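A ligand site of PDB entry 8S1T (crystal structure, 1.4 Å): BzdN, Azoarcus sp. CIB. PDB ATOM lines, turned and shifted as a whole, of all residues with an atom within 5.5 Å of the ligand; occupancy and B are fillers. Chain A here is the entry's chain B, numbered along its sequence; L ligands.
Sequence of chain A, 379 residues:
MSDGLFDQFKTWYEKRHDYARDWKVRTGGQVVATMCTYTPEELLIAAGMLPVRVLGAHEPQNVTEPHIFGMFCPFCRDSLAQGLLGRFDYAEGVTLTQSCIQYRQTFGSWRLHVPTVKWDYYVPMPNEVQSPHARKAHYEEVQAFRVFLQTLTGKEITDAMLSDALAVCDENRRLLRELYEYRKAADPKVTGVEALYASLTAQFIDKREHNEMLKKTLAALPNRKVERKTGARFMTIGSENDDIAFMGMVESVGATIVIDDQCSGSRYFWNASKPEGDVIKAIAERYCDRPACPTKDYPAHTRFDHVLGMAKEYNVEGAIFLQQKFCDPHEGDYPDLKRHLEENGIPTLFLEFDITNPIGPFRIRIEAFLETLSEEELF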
ATOM      1  N   CYS A  36      26.714 -15.901 -18.267  1.00  0.00           N
ATOM      2  CA  CYS A  36      27.497 -17.118 -18.478  1.00  0.00           C
ATOM      3  C   CYS A  36      27.621 -17.965 -17.210  1.00  0.00           C
ATOM      4  O   CYS A  36      27.809 -17.469 -16.072  1.00  0.00           O
ATOM      5  CB  CYS A  36      28.886 -16.857 -19.091  1.00  0.00           C
ATOM      6  SG  CYS A  36      29.855 -18.382 -19.415  1.00  0.00           S
ATOM      7  N   THR A  37      27.579 -19.261 -17.396  1.00  0.00           N
ATOM      8  CA  THR A  37      27.494 -20.198 -16.296  1.00  0.00           C
ATOM      9  C   THR A  37      28.819 -20.354 -15.553  1.00  0.00           C
ATOM     10  O   THR A  37      28.881 -21.099 -14.568  1.00  0.00           O
ATOM     11  CB  THR A  37      27.082 -21.558 -16.848  1.00  0.00           C
ATOM     12  OG1 THR A  37      27.961 -21.877 -17.946  1.00  0.00           O
ATOM     13  CG2 THR A  37      25.669 -21.501 -17.367  1.00  0.00           C
ATOM     14  N   TYR A  38      29.879 -19.676 -15.991  1.00  0.00           N
ATOM     15  CA  TYR A  38      31.154 -19.753 -15.291  1.00  0.00           C
ATOM     16  C   TYR A  38      31.266 -18.758 -14.132  1.00  0.00           C
ATOM     17  O   TYR A  38      32.282 -18.753 -13.448  1.00  0.00           O
ATOM     18  CB  TYR A  38      32.308 -19.515 -16.268  1.00  0.00           C
ATOM     19  CG  TYR A  38      32.692 -20.752 -17.076  1.00  0.00           C
ATOM     20  CD1 TYR A  38      33.237 -21.854 -16.449  1.00  0.00           C
ATOM     21  CD2 TYR A  38      32.562 -20.783 -18.463  1.00  0.00           C
ATOM     22  CE1 TYR A  38      33.616 -22.981 -17.180  1.00  0.00           C
ATOM     23  CE2 TYR A  38      32.947 -21.890 -19.187  1.00  0.00           C
ATOM     24  CZ  TYR A  38      33.495 -22.978 -18.546  1.00  0.00           C
ATOM     25  OH  TYR A  38      33.893 -24.088 -19.225  1.00  0.00           O
ATOM     26  N   ARG A  53      20.803 -15.487 -13.037  1.00  0.00           N
ATOM     27  CA  ARG A  53      21.336 -15.528 -14.395  1.00  0.00           C
ATOM     28  C   ARG A  53      20.416 -14.812 -15.371  1.00  0.00           C
ATOM     29  O   ARG A  53      19.222 -15.116 -15.455  1.00  0.00           O
ATOM     30  CB  ARG A  53      21.458 -16.990 -14.823  1.00  0.00           C
ATOM     31  CG  ARG A  53      21.860 -17.164 -16.276  1.00  0.00           C
ATOM     32  CD  ARG A  53      23.099 -17.979 -16.435  1.00  0.00           C
ATOM     33  NE  ARG A  53      23.457 -18.052 -17.853  1.00  0.00           N
ATOM     34  CZ  ARG A  53      23.179 -19.045 -18.686  1.00  0.00           C
ATOM     35  NH1 ARG A  53      22.507 -20.129 -18.302  1.00  0.00           N
ATOM     36  NH2 ARG A  53      23.599 -18.958 -19.934  1.00  0.00           N
ATOM     37  N   CYS A  73      24.575 -13.314 -32.036  1.00  0.00           N
ATOM     38  CA  CYS A  73      23.570 -14.320 -31.809  1.00  0.00           C
ATOM     39  C   CYS A  73      22.304 -13.750 -31.169  1.00  0.00           C
ATOM     40  O   CYS A  73      22.337 -12.728 -30.475  1.00  0.00           O
ATOM     41  CB  CYS A  73      24.152 -15.439 -30.939  1.00  0.00           C
ATOM     42  SG  CYS A  73      24.400 -14.961 -29.210  1.00  0.00           S
ATOM     43  N   PHE A  75      20.740 -14.890 -28.591  1.00  0.00           N
ATOM     44  CA  PHE A  75      20.745 -14.984 -27.134  1.00  0.00           C
ATOM     45  C   PHE A  75      21.408 -13.763 -26.519  1.00  0.00           C
ATOM     46  O   PHE A  75      20.884 -13.196 -25.552  1.00  0.00           O
ATOM     47  CB  PHE A  75      21.482 -16.246 -26.703  1.00  0.00           C
ATOM     48  CG  PHE A  75      21.553 -16.440 -25.214  1.00  0.00           C
ATOM     49  CD1 PHE A  75      20.405 -16.351 -24.433  1.00  0.00           C
ATOM     50  CD2 PHE A  75      22.748 -16.738 -24.588  1.00  0.00           C
ATOM     51  CE1 PHE A  75      20.465 -16.543 -23.061  1.00  0.00           C
ATOM     52  CE2 PHE A  75      22.817 -16.933 -23.214  1.00  0.00           C
ATOM     53  CZ  PHE A  75      21.671 -16.846 -22.447  1.00  0.00           C
ATOM     54  N   CYS A  76      22.541 -13.327 -27.085  1.00  0.00           N
ATOM     55  CA  CYS A  76      23.236 -12.180 -26.502  1.00  0.00           C
ATOM     56  C   CYS A  76      22.421 -10.905 -26.652  1.00  0.00           C
ATOM     57  O   CYS A  76      22.469 -10.035 -25.758  1.00  0.00           O
ATOM     58  CB  CYS A  76      24.653 -12.079 -27.057  1.00  0.00           C
ATOM     59  SG  CYS A  76      24.887 -11.247 -28.663  1.00  0.00           S
ATOM     60  N   SER A  99      33.894 -16.111 -21.334  1.00  0.00           N
ATOM     61  CA  SER A  99      33.920 -17.214 -22.278  1.00  0.00           C
ATOM     62  C   SER A  99      33.665 -16.623 -23.660  1.00  0.00           C
ATOM     63  O   SER A  99      34.431 -15.751 -24.107  1.00  0.00           O
ATOM     64  CB  SER A  99      32.917 -18.308 -21.885  1.00  0.00           C
ATOM     65  OG  SER A  99      33.316 -19.532 -22.505  1.00  0.00           O
ATOM     66  N   CYS A 100      32.579 -17.026 -24.309  1.00  0.00           N
ATOM     67  CA  CYS A 100      32.304 -16.532 -25.658  1.00  0.00           C
ATOM     68  C   CYS A 100      32.389 -15.008 -25.778  1.00  0.00           C
ATOM     69  O   CYS A 100      31.848 -14.264 -24.949  1.00  0.00           O
ATOM     70  CB  CYS A 100      30.909 -17.001 -26.055  1.00  0.00           C
ATOM     71  SG  CYS A 100      30.309 -16.282 -27.599  1.00  0.00           S
ATOM     72  N   GLN A 102      31.023 -13.042 -27.922  1.00  0.00           N
ATOM     73  CA  GLN A 102      29.782 -12.350 -28.248  1.00  0.00           C
ATOM     74  C   GLN A 102      29.045 -11.946 -26.978  1.00  0.00           C
ATOM     75  O   GLN A 102      28.440 -10.875 -26.916  1.00  0.00           O
ATOM     76  CB  GLN A 102      28.879 -13.212 -29.128  1.00  0.00           C
ATOM     77  CG  GLN A 102      29.485 -13.643 -30.445  1.00  0.00           C
ATOM     78  CD  GLN A 102      28.432 -14.087 -31.423  1.00  0.00           C
ATOM     79  OE1 GLN A 102      27.242 -13.760 -31.291  1.00  0.00           O
ATOM     80  NE2 GLN A 102      28.850 -14.856 -32.405  1.00  0.00           N
ATOM     81  N   TYR A 103      29.010 -12.858 -25.987  1.00  0.00           N
ATOM     82  CA  TYR A 103      28.329 -12.597 -24.726  1.00  0.00           C
ATOM     83  C   TYR A 103      28.954 -11.428 -24.005  1.00  0.00           C
ATOM     84  O   TYR A 103      28.292 -10.745 -23.233  1.00  0.00           O
ATOM     85  CB  TYR A 103      28.516 -13.830 -23.828  1.00  0.00           C
ATOM     86  CG  TYR A 103      27.404 -14.282 -22.928  1.00  0.00           C
ATOM     87  CD1 TYR A 103      26.555 -13.357 -22.296  1.00  0.00           C
ATOM     88  CD2 TYR A 103      27.253 -15.642 -22.645  1.00  0.00           C
ATOM     89  CE1 TYR A 103      25.538 -13.808 -21.446  1.00  0.00           C
ATOM     90  CE2 TYR A 103      26.241 -16.110 -21.793  1.00  0.00           C
ATOM     91  CZ  TYR A 103      25.394 -15.194 -21.196  1.00  0.00           C
ATOM     92  OH  TYR A 103      24.388 -15.672 -20.335  1.00  0.00           O
ATOM     93  N   GLY A 238      23.500 -27.934 -27.259  1.00  0.00           N
ATOM     94  CA  GLY A 238      23.590 -26.547 -27.689  1.00  0.00           C
ATOM     95  C   GLY A 238      24.304 -25.671 -26.696  1.00  0.00           C
ATOM     96  O   GLY A 238      25.022 -26.138 -25.820  1.00  0.00           O
ATOM     97  N   SER A 239      24.110 -24.367 -26.862  1.00  0.00           N
ATOM     98  CA  SER A 239      24.754 -23.414 -25.978  1.00  0.00           C
ATOM     99  C   SER A 239      23.917 -23.305 -24.714  1.00  0.00           C
ATOM    100  O   SER A 239      24.208 -23.994 -23.734  1.00  0.00           O
ATOM    101  CB  SER A 239      25.004 -22.102 -26.730  1.00  0.00           C
ATOM    102  OG  SER A 239      23.798 -21.548 -27.242  1.00  0.00           O
ATOM    103  N   GLU A 240      22.853 -22.493 -24.751  1.00  0.00           N
ATOM    104  CA  GLU A 240      21.962 -22.276 -23.618  1.00  0.00           C
ATOM    105  C   GLU A 240      20.792 -23.253 -23.618  1.00  0.00           C
ATOM    106  O   GLU A 240      20.589 -23.989 -22.645  1.00  0.00           O
ATOM    107  CB  GLU A 240      21.494 -20.811 -23.615  1.00  0.00           C
ATOM    108  CG  GLU A 240      20.470 -20.409 -22.560  1.00  0.00           C
ATOM    109  CD  GLU A 240      20.826 -20.834 -21.154  1.00  0.00           C
ATOM    110  OE1 GLU A 240      22.033 -21.007 -20.880  1.00  0.00           O
ATOM    111  OE2 GLU A 240      19.900 -20.995 -20.320  1.00  0.00           O
ATOM    112  N   CYS A 263      23.872 -25.285 -21.318  1.00  0.00           N
ATOM    113  CA  CYS A 263      24.072 -24.490 -20.102  1.00  0.00           C
ATOM    114  C   CYS A 263      22.790 -24.214 -19.327  1.00  0.00           C
ATOM    115  O   CYS A 263      22.872 -23.783 -18.157  1.00  0.00           O
ATOM    116  CB  CYS A 263      24.846 -23.210 -20.464  1.00  0.00           C
ATOM    117  SG  CYS A 263      26.618 -23.565 -20.456  1.00  0.00           S
ATOM    118  N   ARG A 267      25.657 -28.691 -18.491  1.00  0.00           N
ATOM    119  CA  ARG A 267      26.936 -28.013 -18.522  1.00  0.00           C
ATOM    120  C   ARG A 267      27.059 -27.023 -17.375  1.00  0.00           C
ATOM    121  O   ARG A 267      28.185 -26.693 -16.980  1.00  0.00           O
ATOM    122  CB  ARG A 267      27.185 -27.348 -19.899  1.00  0.00           C
ATOM    123  CG  ARG A 267      28.679 -27.142 -20.184  1.00  0.00           C
ATOM    124  CD  ARG A 267      28.905 -26.247 -21.432  1.00  0.00           C
ATOM    125  NE  ARG A 267      28.490 -26.954 -22.651  1.00  0.00           N
ATOM    126  CZ  ARG A 267      27.466 -26.618 -23.427  1.00  0.00           C
ATOM    127  NH1 ARG A 267      26.712 -25.562 -23.171  1.00  0.00           N
ATOM    128  NH2 ARG A 267      27.165 -27.372 -24.476  1.00  0.00           N
ATOM    129  N   ARG A 290      35.149 -28.231 -14.885  1.00  0.00           N
ATOM    130  CA  ARG A 290      33.796 -28.416 -15.398  1.00  0.00           C
ATOM    131  C   ARG A 290      33.831 -28.799 -16.876  1.00  0.00           C
ATOM    132  O   ARG A 290      34.724 -28.367 -17.621  1.00  0.00           O
ATOM    133  CB  ARG A 290      33.054 -27.102 -15.267  1.00  0.00           C
ATOM    134  CG  ARG A 290      31.551 -27.208 -15.450  1.00  0.00           C
ATOM    135  CD  ARG A 290      30.887 -25.895 -15.759  1.00  0.00           C
ATOM    136  NE  ARG A 290      31.101 -25.574 -17.179  1.00  0.00           N
ATOM    137  CZ  ARG A 290      30.567 -24.521 -17.786  1.00  0.00           C
ATOM    138  NH1 ARG A 290      29.926 -23.597 -17.108  1.00  0.00           N
ATOM    139  NH2 ARG A 290      30.672 -24.413 -19.105  1.00  0.00           N
ATOM    140  N   CYS A 293      32.850 -25.178 -22.031  1.00  0.00           N
ATOM    141  CA  CYS A 293      32.329 -24.428 -23.171  1.00  0.00           C
ATOM    142  C   CYS A 293      33.197 -24.722 -24.395  1.00  0.00           C
ATOM    143  O   CYS A 293      34.412 -24.878 -24.243  1.00  0.00           O
ATOM    144  CB  CYS A 293      32.456 -22.920 -22.889  1.00  0.00           C
ATOM    145  SG  CYS A 293      31.805 -21.805 -24.164  1.00  0.00           S
ATOM    146  N   PRO A 294      32.631 -24.819 -25.606  1.00  0.00           N
ATOM    147  CA  PRO A 294      33.493 -24.943 -26.800  1.00  0.00           C
ATOM    148  C   PRO A 294      34.609 -23.931 -26.854  1.00  0.00           C
ATOM    149  O   PRO A 294      35.716 -24.277 -27.284  1.00  0.00           O
ATOM    150  CB  PRO A 294      32.495 -24.784 -27.967  1.00  0.00           C
ATOM    151  CG  PRO A 294      31.221 -25.349 -27.427  1.00  0.00           C
ATOM    152  CD  PRO A 294      31.197 -24.894 -25.981  1.00  0.00           C
ATOM    153  N   GLN A 324      21.847 -21.580 -31.880  1.00  0.00           N
ATOM    154  CA  GLN A 324      21.507 -20.184 -32.068  1.00  0.00           C
ATOM    155  C   GLN A 324      22.120 -19.724 -33.366  1.00  0.00           C
ATOM    156  O   GLN A 324      23.244 -20.098 -33.713  1.00  0.00           O
ATOM    157  CB  GLN A 324      22.083 -19.351 -30.941  1.00  0.00           C
ATOM    158  CG  GLN A 324      21.427 -19.681 -29.608  1.00  0.00           C
ATOM    159  CD  GLN A 324      20.022 -19.137 -29.511  1.00  0.00           C
ATOM    160  OE1 GLN A 324      19.816 -17.925 -29.564  1.00  0.00           O
ATOM    161  NE2 GLN A 324      19.052 -20.007 -29.375  1.00  0.00           N
ATOM    162  N   PHE A 326      24.243 -17.735 -35.767  1.00  0.00           N
ATOM    163  CA  PHE A 326      25.506 -17.001 -35.648  1.00  0.00           C
ATOM    164  C   PHE A 326      26.418 -17.500 -34.533  1.00  0.00           C
ATOM    165  O   PHE A 326      27.410 -16.842 -34.219  1.00  0.00           O
ATOM    166  CB  PHE A 326      25.275 -15.481 -35.521  1.00  0.00           C
ATOM    167  CG  PHE A 326      24.458 -14.898 -36.629  1.00  0.00           C
ATOM    168  CD1 PHE A 326      24.854 -15.060 -37.962  1.00  0.00           C
ATOM    169  CD2 PHE A 326      23.329 -14.176 -36.367  1.00  0.00           C
ATOM    170  CE1 PHE A 326      24.113 -14.527 -38.990  1.00  0.00           C
ATOM    171  CE2 PHE A 326      22.599 -13.609 -37.389  1.00  0.00           C
ATOM    172  CZ  PHE A 326      22.978 -13.780 -38.710  1.00  0.00           C
ATOM    173  N   CYS A 327      26.122 -18.607 -33.882  1.00  0.00           N
ATOM    174  CA  CYS A 327      26.886 -19.033 -32.694  1.00  0.00           C
ATOM    175  C   CYS A 327      28.244 -19.654 -33.050  1.00  0.00           C
ATOM    176  O   CYS A 327      28.352 -20.837 -33.358  1.00  0.00           O
ATOM    177  CB  CYS A 327      26.044 -20.021 -31.891  1.00  0.00           C
ATOM    178  SG  CYS A 327      26.844 -20.673 -30.414  1.00  0.00           S
ATOM    179  N   ASP A 328      29.287 -18.832 -33.035  1.00  0.00           N
ATOM    180  CA  ASP A 328      30.587 -19.290 -33.507  1.00  0.00           C
ATOM    181  C   ASP A 328      31.186 -20.425 -32.712  1.00  0.00           C
ATOM    182  O   ASP A 328      31.739 -21.351 -33.324  1.00  0.00           O
ATOM    183  CB  ASP A 328      31.567 -18.113 -33.543  1.00  0.00           C
ATOM    184  CG  ASP A 328      31.156 -17.061 -34.540  1.00  0.00           C
ATOM    185  OD1 ASP A 328      31.322 -17.323 -35.764  1.00  0.00           O
ATOM    186  OD2 ASP A 328      30.677 -15.963 -34.152  1.00  0.00           O
ATOM    187  N   PRO A 329      31.135 -20.439 -31.370  1.00  0.00           N
ATOM    188  CA  PRO A 329      31.849 -21.514 -30.663  1.00  0.00           C
ATOM    189  C   PRO A 329      31.225 -22.872 -30.996  1.00  0.00           C
ATOM    190  O   PRO A 329      31.943 -23.846 -31.243  1.00  0.00           O
ATOM    191  CB  PRO A 329      31.758 -21.101 -29.174  1.00  0.00           C
ATOM    192  CG  PRO A 329      31.501 -19.620 -29.220  1.00  0.00           C
ATOM    193  CD  PRO A 329      30.637 -19.414 -30.434  1.00  0.00           C
ATOM    194  N   HIS A 330      29.912 -22.934 -31.060  1.00  0.00           N
ATOM    195  CA  HIS A 330      29.265 -24.222 -31.302  1.00  0.00           C
ATOM    196  C   HIS A 330      29.281 -24.567 -32.772  1.00  0.00           C
ATOM    197  O   HIS A 330      29.352 -25.759 -33.135  1.00  0.00           O
ATOM    198  CB  HIS A 330      27.864 -24.146 -30.702  1.00  0.00           C
ATOM    199  CG  HIS A 330      27.877 -24.113 -29.203  1.00  0.00           C
ATOM    200  ND1 HIS A 330      27.630 -25.245 -28.450  1.00  0.00           N
ATOM    201  CD2 HIS A 330      28.138 -23.113 -28.316  1.00  0.00           C
ATOM    202  CE1 HIS A 330      27.740 -24.943 -27.166  1.00  0.00           C
ATOM    203  NE2 HIS A 330      28.028 -23.666 -27.056  1.00  0.00           N
HETATM  204  S1  LIG L   1      27.421 -16.992 -29.837  1.00  0.00           S
HETATM  205  S2  LIG L   1      26.652 -16.078 -26.359  1.00  0.00           S
HETATM  206  S3  LIG L   1      28.085 -19.407 -27.134  1.00  0.00           S
HETATM  207  S4  LIG L   1      24.639 -18.584 -28.004  1.00  0.00           S
HETATM  208  S5  LIG L   1      27.768 -22.098 -23.961  1.00  0.00           S
HETATM  209  S6  LIG L   1      26.680 -19.910 -21.103  1.00  0.00           S
HETATM  210  S7  LIG L   1      29.301 -18.885 -23.347  1.00  0.00           S
HETATM  211  S8  LIG L   1      29.811 -21.643 -21.056  1.00  0.00           S
HETATM  212  S9  LIG L   1      25.473 -19.076 -24.276  1.00  0.00           S
HETATM  213 FE1  LIG L   1      26.187 -18.321 -26.299  1.00  0.00          FE
HETATM  214 FE2  LIG L   1      26.726 -18.971 -28.907  1.00  0.00          FE
HETATM  215 FE3  LIG L   1      25.694 -16.556 -28.360  1.00  0.00          FE
HETATM  216 FE4  LIG L   1      28.214 -17.159 -27.668  1.00  0.00          FE
HETATM  217 FE5  LIG L   1      28.901 -19.521 -21.135  1.00  0.00          FE
HETATM  218 FE6  LIG L   1      29.706 -21.149 -23.290  1.00  0.00          FE
HETATM  219 FE7  LIG L   1      27.659 -21.889 -21.655  1.00  0.00          FE
HETATM  220 FE8  LIG L   1      27.268 -19.906 -23.338  1.00  0.00          FE
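Tyr 38 touches the ligand.
Phe 75 touches the ligand (CE2 to S9, 3.6 Å).
CB of Ser 99 touches S7 of the ligand, 3.9 Å away.
Tyr 103 touches the ligand (CD2 to S2, 3.8 Å).
CG of Gln 324 touches S4 of the ligand (3.8 Å).
Hydrophobic or aromatic side chains that line the ligand: Tyr 38, Phe 75, Tyr 103 and His 330.
Of the 25 residues printed, 18 come within 4 Å of the ligand.
The side-chain hydroxyl of Tyr 38 sits at hydrogen-bond distance from the backbone NH of Cys 293, 3.2 Å away.
NH2 of Arg 53 sits at hydrogen-bond distance from OH of Tyr 103, 3.4 Å away.
The guanidinium group (NH1) of Arg 267 lies close to the side-chain sulfur (SG) of Cys 263, at 3.4 Å.
NH2 of Arg 290 sits close to OH of Tyr 38 (3.2 Å).
NH2 of Arg 267 sits at hydrogen-bond distance from O of Gly 238 (2.8 Å).
The side-chain carboxylate of Asp 328 lies within hydrogen-bond range of the side-chain amide nitrogen of Gln 102, at 2.8 Å.
The backbone NH of Cys 73 lies within hydrogen-bond range of the side-chain amide oxygen of Gln 102 (2.8 Å).
The side-chain carboxylate (OE1) of Glu 240 lies within salt-bridge range of the guanidinium group (NH2) of Arg 53 (2.7 Å).
The side-chain sulfur (SG) of Cys 327 binds an iron atom (FE2) of the ligand, at 2.3 Å.
FE4 of the ligand is bound by SG of Cys 100, 2.3 Å away.
SG of Cys 36 binds FE5 of the ligand, at 2.3 Å.
OE1 of Gln 102 lies close to S1 of the ligand.
S5 of the ligand sits close to NE2 of His 330, 3.5 Å away.
OG of Ser 239 lies close to S4 of the ligand (3.2 Å).
SG of Cys 263 binds FE7 of the ligand, 2.3 Å away.
A sulfur (S8) of the ligand sits close to the side-chain hydroxyl (OG1) of Thr 37, at 3.6 Å.
The side-chain sulfur (SG) of Cys 73 binds an iron atom (FE3) of the ligand, at 2.2 Å.
The side-chain sulfur (SG) of Cys 293 binds an iron atom (FE6) of the ligand (2.4 Å).
NH1 of Arg 267 lies close to S5 of the ligand (3.7 Å).
The guanidinium group (NH2) of Arg 53 lies close to a sulfur (S6) of the ligand (3.4 Å).
The guanidinium group (NH2) of Arg 290 sits close to a sulfur (S8) of the ligand (3.5 Å).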
